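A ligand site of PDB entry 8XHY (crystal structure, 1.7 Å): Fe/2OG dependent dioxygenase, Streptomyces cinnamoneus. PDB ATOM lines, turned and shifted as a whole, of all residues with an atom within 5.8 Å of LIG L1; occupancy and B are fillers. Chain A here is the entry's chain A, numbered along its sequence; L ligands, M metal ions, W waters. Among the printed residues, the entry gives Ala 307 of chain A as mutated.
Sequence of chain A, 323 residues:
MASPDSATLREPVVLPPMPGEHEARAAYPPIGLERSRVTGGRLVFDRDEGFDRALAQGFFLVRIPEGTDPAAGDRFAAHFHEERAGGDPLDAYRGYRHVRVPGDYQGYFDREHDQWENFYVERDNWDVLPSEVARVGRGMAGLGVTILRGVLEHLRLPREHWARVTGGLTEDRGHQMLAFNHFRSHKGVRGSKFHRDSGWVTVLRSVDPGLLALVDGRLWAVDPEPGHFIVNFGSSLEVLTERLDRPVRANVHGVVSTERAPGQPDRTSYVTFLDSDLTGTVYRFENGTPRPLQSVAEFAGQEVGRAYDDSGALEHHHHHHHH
OH of Tyr 120 lies within hydrogen-bond range of OH of Tyr 308, 2.6 Å away.
OG1 of Thr 202 is in hydrogen-bond range of OD2 of Asp 197, at 2.8 Å.
The backbone NH of Phe 273 is in hydrogen-bond range of the backbone carbonyl oxygen of Met 177 (2.9 Å).
The side-chain hydroxyl (OH) of Tyr 308 sits close to the guanidinium group (NH2) of Arg 111 (3.4 Å).
The backbone carbonyl oxygen (O) of His 175 lies within hydrogen-bond range of the backbone NH (N) of Asp 275 (2.9 Å).
OG of Ser 198 lies within hydrogen-bond range of OD2 of Asp 275 (2.5 Å).
The side-chain carboxylate (OD2) of Asp 275 lies close to the backbone NH (N) of Gly 199, at 3.3 Å.
Merely in contact with LIG L1: Asp 197, Ala 307, Tyr 120, Asp 275, Ala 300, Phe 273, His 175, Val 304, His 195, Arg 196, Met 177 and Trp 116.
Hydrophobic or aromatic side chains that line LIG L1: Trp 116, Tyr 120, His 175, Met 177, His 195, Phe 273, Ala 300, Val 304, Ala 307 and Tyr 308.
An oxygen (O2) of LIG L1 is in hydrogen-bond range of the backbone NH of Ser 198, at 2.9 Å.
The side-chain hydroxyl (OG) of Ser 198 sits at hydrogen-bond distance from a nitrogen (N2) of LIG L1, 3.0 Å away.
OH of Tyr 308 sits at hydrogen-bond distance from N1 of LIG L1, at 2.9 Å.
Water W1 lies within hydrogen-bond range of O2 of LIG L1 (2.8 Å), OD1 of Asp 275 (2.9 Å), N of Gly 199 (2.9 Å) and OG of Ser 198 (3.3 Å).
Water W2 lies within hydrogen-bond range of an oxygen (O1) of LIG L1 (2.8 Å), the guanidinium group (NH2) of Arg 111 (3.1 Å) and the backbone carbonyl oxygen (O) of Tyr 105 (3.5 Å).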
ATOM      1  N   ASP A 104     -10.804  12.259   5.174  1.00  0.00           N
ATOM      2  CA  ASP A 104     -10.376  11.571   6.379  1.00  0.00           C
ATOM      3  C   ASP A 104     -11.141  10.282   6.558  1.00  0.00           C
ATOM      4  O   ASP A 104     -12.374  10.258   6.420  1.00  0.00           O
ATOM      5  CB  ASP A 104     -10.606  12.454   7.616  1.00  0.00           C
ATOM      6  CG  ASP A 104      -9.720  13.687   7.636  1.00  0.00           C
ATOM      7  OD1 ASP A 104      -8.676  13.677   6.942  1.00  0.00           O
ATOM      8  OD2 ASP A 104     -10.063  14.650   8.357  1.00  0.00           O
ATOM      9  N   TYR A 105     -10.419   9.213   6.895  1.00  0.00           N
ATOM     10  CA  TYR A 105     -10.968   7.891   7.243  1.00  0.00           C
ATOM     11  C   TYR A 105     -11.539   7.152   6.053  1.00  0.00           C
ATOM     12  O   TYR A 105     -12.250   6.161   6.244  1.00  0.00           O
ATOM     13  CB  TYR A 105     -12.048   8.000   8.336  1.00  0.00           C
ATOM     14  CG  TYR A 105     -11.525   8.846   9.480  1.00  0.00           C
ATOM     15  CD1 TYR A 105     -12.125  10.067   9.825  1.00  0.00           C
ATOM     16  CD2 TYR A 105     -10.411   8.439  10.183  1.00  0.00           C
ATOM     17  CE1 TYR A 105     -11.610  10.848  10.870  1.00  0.00           C
ATOM     18  CE2 TYR A 105      -9.892   9.223  11.248  1.00  0.00           C
ATOM     19  CZ  TYR A 105     -10.512  10.415  11.582  1.00  0.00           C
ATOM     20  OH  TYR A 105     -10.005  11.200  12.638  1.00  0.00           O
ATOM     21  N   ARG A 111      -4.991  -3.017   7.854  1.00  0.00           N
ATOM     22  CA  ARG A 111      -4.851  -2.931   9.303  1.00  0.00           C
ATOM     23  C   ARG A 111      -3.745  -3.867   9.758  1.00  0.00           C
ATOM     24  O   ARG A 111      -3.791  -5.091   9.538  1.00  0.00           O
ATOM     25  CB  ARG A 111      -6.180  -3.289   9.977  1.00  0.00           C
ATOM     26  CG  ARG A 111      -7.378  -2.462   9.540  1.00  0.00           C
ATOM     27  CD  ARG A 111      -7.210  -0.955   9.659  1.00  0.00           C
ATOM     28  NE  ARG A 111      -8.417  -0.260   9.199  1.00  0.00           N
ATOM     29  CZ  ARG A 111      -8.588   1.065   9.257  1.00  0.00           C
ATOM     30  NH1 ARG A 111      -7.610   1.831   9.754  1.00  0.00           N
ATOM     31  NH2 ARG A 111      -9.709   1.615   8.814  1.00  0.00           N
ATOM     32  N   TRP A 116      -8.875  -7.929   9.272  1.00  0.00           N
ATOM     33  CA  TRP A 116      -9.590  -7.238   8.207  1.00  0.00           C
ATOM     34  C   TRP A 116      -8.696  -6.231   7.508  1.00  0.00           C
ATOM     35  O   TRP A 116      -7.769  -5.675   8.089  1.00  0.00           O
ATOM     36  CB  TRP A 116     -10.875  -6.561   8.685  1.00  0.00           C
ATOM     37  CG  TRP A 116     -10.825  -5.522   9.771  1.00  0.00           C
ATOM     38  CD1 TRP A 116      -9.731  -4.978  10.390  1.00  0.00           C
ATOM     39  CD2 TRP A 116     -11.975  -4.933  10.380  1.00  0.00           C
ATOM     40  NE1 TRP A 116     -10.140  -4.083  11.363  1.00  0.00           N
ATOM     41  CE2 TRP A 116     -11.514  -4.028  11.356  1.00  0.00           C
ATOM     42  CE3 TRP A 116     -13.352  -5.075  10.177  1.00  0.00           C
ATOM     43  CZ2 TRP A 116     -12.397  -3.260  12.143  1.00  0.00           C
ATOM     44  CZ3 TRP A 116     -14.237  -4.311  10.944  1.00  0.00           C
ATOM     45  CH2 TRP A 116     -13.750  -3.417  11.908  1.00  0.00           C
ATOM     46  N   TYR A 120     -13.332   1.947   2.529  1.00  0.00           N
ATOM     47  CA  TYR A 120     -14.327   2.831   3.113  1.00  0.00           C
ATOM     48  C   TYR A 120     -14.636   3.963   2.147  1.00  0.00           C
ATOM     49  O   TYR A 120     -13.718   4.639   1.680  1.00  0.00           O
ATOM     50  CB  TYR A 120     -13.820   3.449   4.432  1.00  0.00           C
ATOM     51  CG  TYR A 120     -13.707   2.528   5.654  1.00  0.00           C
ATOM     52  CD1 TYR A 120     -14.210   1.233   5.658  1.00  0.00           C
ATOM     53  CD2 TYR A 120     -13.116   2.986   6.807  1.00  0.00           C
ATOM     54  CE1 TYR A 120     -14.121   0.417   6.768  1.00  0.00           C
ATOM     55  CE2 TYR A 120     -13.013   2.166   7.958  1.00  0.00           C
ATOM     56  CZ  TYR A 120     -13.523   0.897   7.926  1.00  0.00           C
ATOM     57  OH  TYR A 120     -13.436   0.099   9.064  1.00  0.00           O
ATOM     58  N   HIS A 175     -22.371  12.268   7.473  1.00  0.00           N
ATOM     59  CA  HIS A 175     -21.263  11.518   6.904  1.00  0.00           C
ATOM     60  C   HIS A 175     -21.778  10.072   6.797  1.00  0.00           C
ATOM     61  O   HIS A 175     -21.940   9.368   7.800  1.00  0.00           O
ATOM     62  CB  HIS A 175     -20.014  11.664   7.790  1.00  0.00           C
ATOM     63  CG  HIS A 175     -18.761  11.058   7.219  1.00  0.00           C
ATOM     64  ND1 HIS A 175     -18.495   9.701   7.257  1.00  0.00           N
ATOM     65  CD2 HIS A 175     -17.673  11.633   6.653  1.00  0.00           C
ATOM     66  CE1 HIS A 175     -17.320   9.472   6.712  1.00  0.00           C
ATOM     67  NE2 HIS A 175     -16.803  10.622   6.323  1.00  0.00           N
ATOM     68  N   MET A 177     -21.271   6.453   5.246  1.00  0.00           N
ATOM     69  CA  MET A 177     -20.111   5.769   4.697  1.00  0.00           C
ATOM     70  C   MET A 177     -20.377   4.290   4.463  1.00  0.00           C
ATOM     71  O   MET A 177     -20.801   3.578   5.376  1.00  0.00           O
ATOM     72  CB  MET A 177     -18.907   5.973   5.598  1.00  0.00           C
ATOM     73  CG  MET A 177     -17.630   5.464   4.889  1.00  0.00           C
ATOM     74  SD  MET A 177     -16.095   6.089   5.606  1.00  0.00           S
ATOM     75  CE  MET A 177     -16.016   5.166   7.124  1.00  0.00           C
ATOM     76  N   HIS A 195     -14.252  -2.971  19.531  1.00  0.00           N
ATOM     77  CA  HIS A 195     -14.438  -1.551  19.281  1.00  0.00           C
ATOM     78  C   HIS A 195     -15.912  -1.178  19.461  1.00  0.00           C
ATOM     79  O   HIS A 195     -16.796  -2.033  19.422  1.00  0.00           O
ATOM     80  CB  HIS A 195     -13.984  -1.171  17.844  1.00  0.00           C
ATOM     81  CG  HIS A 195     -14.802  -1.828  16.770  1.00  0.00           C
ATOM     82  ND1 HIS A 195     -14.564  -3.104  16.298  1.00  0.00           N
ATOM     83  CD2 HIS A 195     -15.879  -1.370  16.092  1.00  0.00           C
ATOM     84  CE1 HIS A 195     -15.443  -3.401  15.365  1.00  0.00           C
ATOM     85  NE2 HIS A 195     -16.249  -2.359  15.212  1.00  0.00           N
ATOM     86  N   ARG A 196     -16.149   0.112  19.692  1.00  0.00           N
ATOM     87  CA  ARG A 196     -17.448   0.702  19.435  1.00  0.00           C
ATOM     88  C   ARG A 196     -17.400   1.423  18.094  1.00  0.00           C
ATOM     89  O   ARG A 196     -16.373   2.010  17.722  1.00  0.00           O
ATOM     90  CB  ARG A 196     -17.859   1.700  20.521  1.00  0.00           C
ATOM     91  CG  ARG A 196     -18.096   0.981  21.850  1.00  0.00           C
ATOM     92  CD  ARG A 196     -18.489   2.000  22.950  1.00  0.00           C
ATOM     93  NE  ARG A 196     -17.276   2.495  23.539  1.00  0.00           N
ATOM     94  CZ  ARG A 196     -17.001   2.521  24.845  1.00  0.00           C
ATOM     95  NH1 ARG A 196     -17.906   2.135  25.756  1.00  0.00           N
ATOM     96  NH2 ARG A 196     -15.834   2.997  25.228  1.00  0.00           N
ATOM     97  N   ASP A 197     -18.489   1.347  17.355  1.00  0.00           N
ATOM     98  CA  ASP A 197     -18.589   2.161  16.143  1.00  0.00           C
ATOM     99  C   ASP A 197     -18.770   3.601  16.602  1.00  0.00           C
ATOM    100  O   ASP A 197     -19.314   3.843  17.674  1.00  0.00           O
ATOM    101  CB  ASP A 197     -19.776   1.748  15.273  1.00  0.00           C
ATOM    102  CG  ASP A 197     -19.675   0.309  14.734  1.00  0.00           C
ATOM    103  OD1 ASP A 197     -18.559  -0.258  14.767  1.00  0.00           O
ATOM    104  OD2 ASP A 197     -20.702  -0.229  14.248  1.00  0.00           O
ATOM    105  N   SER A 198     -18.268   4.547  15.814  1.00  0.00           N
ATOM    106  CA  SER A 198     -18.142   5.930  16.277  1.00  0.00           C
ATOM    107  C   SER A 198     -19.456   6.704  16.190  1.00  0.00           C
ATOM    108  O   SER A 198     -19.646   7.684  16.924  1.00  0.00           O
ATOM    109  CB  SER A 198     -17.072   6.652  15.434  1.00  0.00           C
ATOM    110  OG  SER A 198     -17.492   6.804  14.052  1.00  0.00           O
ATOM    111  N   GLY A 199     -20.358   6.268  15.311  1.00  0.00           N
ATOM    112  CA  GLY A 199     -21.441   7.130  14.879  1.00  0.00           C
ATOM    113  C   GLY A 199     -22.778   6.925  15.562  1.00  0.00           C
ATOM    114  O   GLY A 199     -22.847   6.938  16.802  1.00  0.00           O
ATOM    115  N   THR A 202     -25.440   1.809  12.801  1.00  0.00           N
ATOM    116  CA  THR A 202     -24.692   0.999  11.837  1.00  0.00           C
ATOM    117  C   THR A 202     -25.609  -0.085  11.284  1.00  0.00           C
ATOM    118  O   THR A 202     -26.267  -0.796  12.047  1.00  0.00           O
ATOM    119  CB  THR A 202     -23.476   0.333  12.507  1.00  0.00           C
ATOM    120  OG1 THR A 202     -22.630   1.344  13.077  1.00  0.00           O
ATOM    121  CG2 THR A 202     -22.632  -0.519  11.475  1.00  0.00           C
ATOM    122  N   PHE A 273     -21.998   3.080   7.941  1.00  0.00           N
ATOM    123  CA  PHE A 273     -21.829   3.867   9.164  1.00  0.00           C
ATOM    124  C   PHE A 273     -22.474   5.237   8.958  1.00  0.00           C
ATOM    125  O   PHE A 273     -22.183   5.919   7.959  1.00  0.00           O
ATOM    126  CB  PHE A 273     -20.346   4.085   9.479  1.00  0.00           C
ATOM    127  CG  PHE A 273     -19.545   2.833   9.760  1.00  0.00           C
ATOM    128  CD1 PHE A 273     -19.830   2.020  10.878  1.00  0.00           C
ATOM    129  CD2 PHE A 273     -18.414   2.534   8.979  1.00  0.00           C
ATOM    130  CE1 PHE A 273     -19.049   0.914  11.173  1.00  0.00           C
ATOM    131  CE2 PHE A 273     -17.602   1.389   9.276  1.00  0.00           C
ATOM    132  CZ  PHE A 273     -17.923   0.597  10.396  1.00  0.00           C
ATOM    133  N   ASP A 275     -22.345   8.753  10.583  1.00  0.00           N
ATOM    134  CA  ASP A 275     -21.637   9.638  11.482  1.00  0.00           C
ATOM    135  C   ASP A 275     -22.129  11.064  11.280  1.00  0.00           C
ATOM    136  O   ASP A 275     -22.667  11.417  10.236  1.00  0.00           O
ATOM    137  CB  ASP A 275     -20.116   9.559  11.253  1.00  0.00           C
ATOM    138  CG  ASP A 275     -19.482   8.367  11.982  1.00  0.00           C
ATOM    139  OD1 ASP A 275     -19.333   7.283  11.339  1.00  0.00           O
ATOM    140  OD2 ASP A 275     -19.141   8.511  13.191  1.00  0.00           O
ATOM    141  N   LEU A 278     -18.342  15.789   9.741  1.00  0.00           N
ATOM    142  CA  LEU A 278     -17.051  15.816  10.448  1.00  0.00           C
ATOM    143  C   LEU A 278     -16.610  17.235  10.832  1.00  0.00           C
ATOM    144  O   LEU A 278     -15.645  17.374  11.609  1.00  0.00           O
ATOM    145  CB  LEU A 278     -15.955  15.146   9.637  1.00  0.00           C
ATOM    146  CG  LEU A 278     -16.192  13.669   9.274  1.00  0.00           C
ATOM    147  CD1 LEU A 278     -14.990  13.115   8.566  1.00  0.00           C
ATOM    148  CD2 LEU A 278     -16.499  12.809  10.519  1.00  0.00           C
ATOM    149  N   ALA A 300     -13.748  12.015  16.401  1.00  0.00           N
ATOM    150  CA  ALA A 300     -13.440  10.985  15.421  1.00  0.00           C
ATOM    151  C   ALA A 300     -12.017  10.484  15.608  1.00  0.00           C
ATOM    152  O   ALA A 300     -11.779   9.264  15.610  1.00  0.00           O
ATOM    153  CB  ALA A 300     -13.611  11.517  13.990  1.00  0.00           C
ATOM    154  N   GLU A 303     -11.899   8.249  18.618  1.00  0.00           N
ATOM    155  CA  GLU A 303     -12.584   6.969  18.534  1.00  0.00           C
ATOM    156  C   GLU A 303     -11.913   6.050  17.523  1.00  0.00           C
ATOM    157  O   GLU A 303     -11.793   4.845  17.759  1.00  0.00           O
ATOM    158  CB  GLU A 303     -14.068   7.188  18.220  1.00  0.00           C
ATOM    159  CG  GLU A 303     -14.789   7.860  19.425  1.00  0.00           C
ATOM    160  CD  GLU A 303     -14.643   7.048  20.774  1.00  0.00           C
ATOM    161  OE1 GLU A 303     -15.211   5.933  20.874  1.00  0.00           O
ATOM    162  OE2 GLU A 303     -13.943   7.521  21.720  1.00  0.00           O
ATOM    163  N   VAL A 304     -11.459   6.616  16.399  1.00  0.00           N
ATOM    164  CA  VAL A 304     -10.693   5.826  15.449  1.00  0.00           C
ATOM    165  C   VAL A 304      -9.378   5.385  16.055  1.00  0.00           C
ATOM    166  O   VAL A 304      -8.915   4.263  15.835  1.00  0.00           O
ATOM    167  CB  VAL A 304     -10.463   6.592  14.132  1.00  0.00           C
ATOM    168  CG1 VAL A 304      -9.465   5.830  13.232  1.00  0.00           C
ATOM    169  CG2 VAL A 304     -11.777   6.747  13.401  1.00  0.00           C
ATOM    170  N   ALA A 307     -10.176   2.269  18.054  1.00  0.00           N
ATOM    171  CA  ALA A 307     -10.775   1.148  17.343  1.00  0.00           C
ATOM    172  C   ALA A 307      -9.725   0.335  16.590  1.00  0.00           C
ATOM    173  O   ALA A 307      -9.933  -0.858  16.328  1.00  0.00           O
ATOM    174  CB  ALA A 307     -11.826   1.660  16.359  1.00  0.00           C
ATOM    175  N   TYR A 308      -8.599   0.954  16.277  1.00  0.00           N
ATOM    176  CA  TYR A 308      -7.514   0.287  15.550  1.00  0.00           C
ATOM    177  C   TYR A 308      -6.218   0.577  16.294  1.00  0.00           C
ATOM    178  O   TYR A 308      -6.096   1.617  16.955  1.00  0.00           O
ATOM    179  CB  TYR A 308      -7.390   0.761  14.105  1.00  0.00           C
ATOM    180  CG  TYR A 308      -8.689   0.851  13.303  1.00  0.00           C
ATOM    181  CD1 TYR A 308      -9.213  -0.279  12.633  1.00  0.00           C
ATOM    182  CD2 TYR A 308      -9.378   2.066  13.198  1.00  0.00           C
ATOM    183  CE1 TYR A 308     -10.418  -0.176  11.895  1.00  0.00           C
ATOM    184  CE2 TYR A 308     -10.547   2.181  12.462  1.00  0.00           C
ATOM    185  CZ  TYR A 308     -11.057   1.068  11.786  1.00  0.00           C
ATOM    186  OH  TYR A 308     -12.212   1.235  11.058  1.00  0.00           O
HETATM  187  C1  LIG L   1     -14.792   6.867  11.347  1.00  0.00           C
HETATM  188  C2  LIG L   1     -16.140   8.322   9.839  1.00  0.00           C
HETATM  189  C3  LIG L   1     -15.628   2.667  12.092  1.00  0.00           C
HETATM  190  C4  LIG L   1     -16.594   3.760  12.482  1.00  0.00           C
HETATM  191  C5  LIG L   1     -15.365   5.463  10.971  1.00  0.00           C
HETATM  192  C6  LIG L   1     -14.226   4.431  10.871  1.00  0.00           C
HETATM  193  C7  LIG L   1     -15.337   1.723  13.280  1.00  0.00           C
HETATM  194  C8  LIG L   1     -14.852   0.273  12.753  1.00  0.00           C
HETATM  195  C9  LIG L   1     -14.284   2.356  14.166  1.00  0.00           C
HETATM  196  C10 LIG L   1     -14.569   3.806  14.815  1.00  0.00           C
HETATM  197  C11 LIG L   1     -15.926   7.953  11.331  1.00  0.00           C
HETATM  198  C12 LIG L   1     -15.493   9.187  12.149  1.00  0.00           C
HETATM  199  N1  LIG L   1     -14.403   3.170  11.425  1.00  0.00           N
HETATM  200  N2  LIG L   1     -16.443   5.037  11.928  1.00  0.00           N
HETATM  201  O1  LIG L   1     -13.175   4.688  10.316  1.00  0.00           O
HETATM  202  O2  LIG L   1     -17.525   3.515  13.253  1.00  0.00           O
HETATM  203  C1  LG2 L   2     -17.499  -3.093  11.626  1.00  0.00           C
HETATM  204  O1  LG2 L   2     -17.322  -3.013  10.360  1.00  0.00           O
HETATM  205  O2  LG2 L   2     -17.398  -2.076  12.347  1.00  0.00           O
HETATM  206  C2  LG2 L   2     -17.868  -4.365  12.276  1.00  0.00           C
HETATM  207  O3  LG2 L   2     -18.034  -4.435  13.508  1.00  0.00           O
HETATM  208  C3  LG2 L   2     -18.044  -5.600  11.417  1.00  0.00           C
HETATM  209  C4  LG2 L   2     -18.812  -6.713  12.118  1.00  0.00           C
HETATM  210  C5  LG2 L   2     -18.822  -8.009  11.318  1.00  0.00           C
HETATM  211  O4  LG2 L   2     -18.073  -8.151  10.348  1.00  0.00           O
HETATM  212  O5  LG2 L   2     -19.604  -8.940  11.673  1.00  0.00           O
HETATM  213 FE    FE M   1     -18.173  -2.399  14.268  1.00  0.00          FE
HETATM  214  O   HOH W   1     -19.907   4.915  12.823  1.00  0.00           O
HETATM  215  O   HOH W   2     -10.761   4.536   8.903  1.00  0.00           O
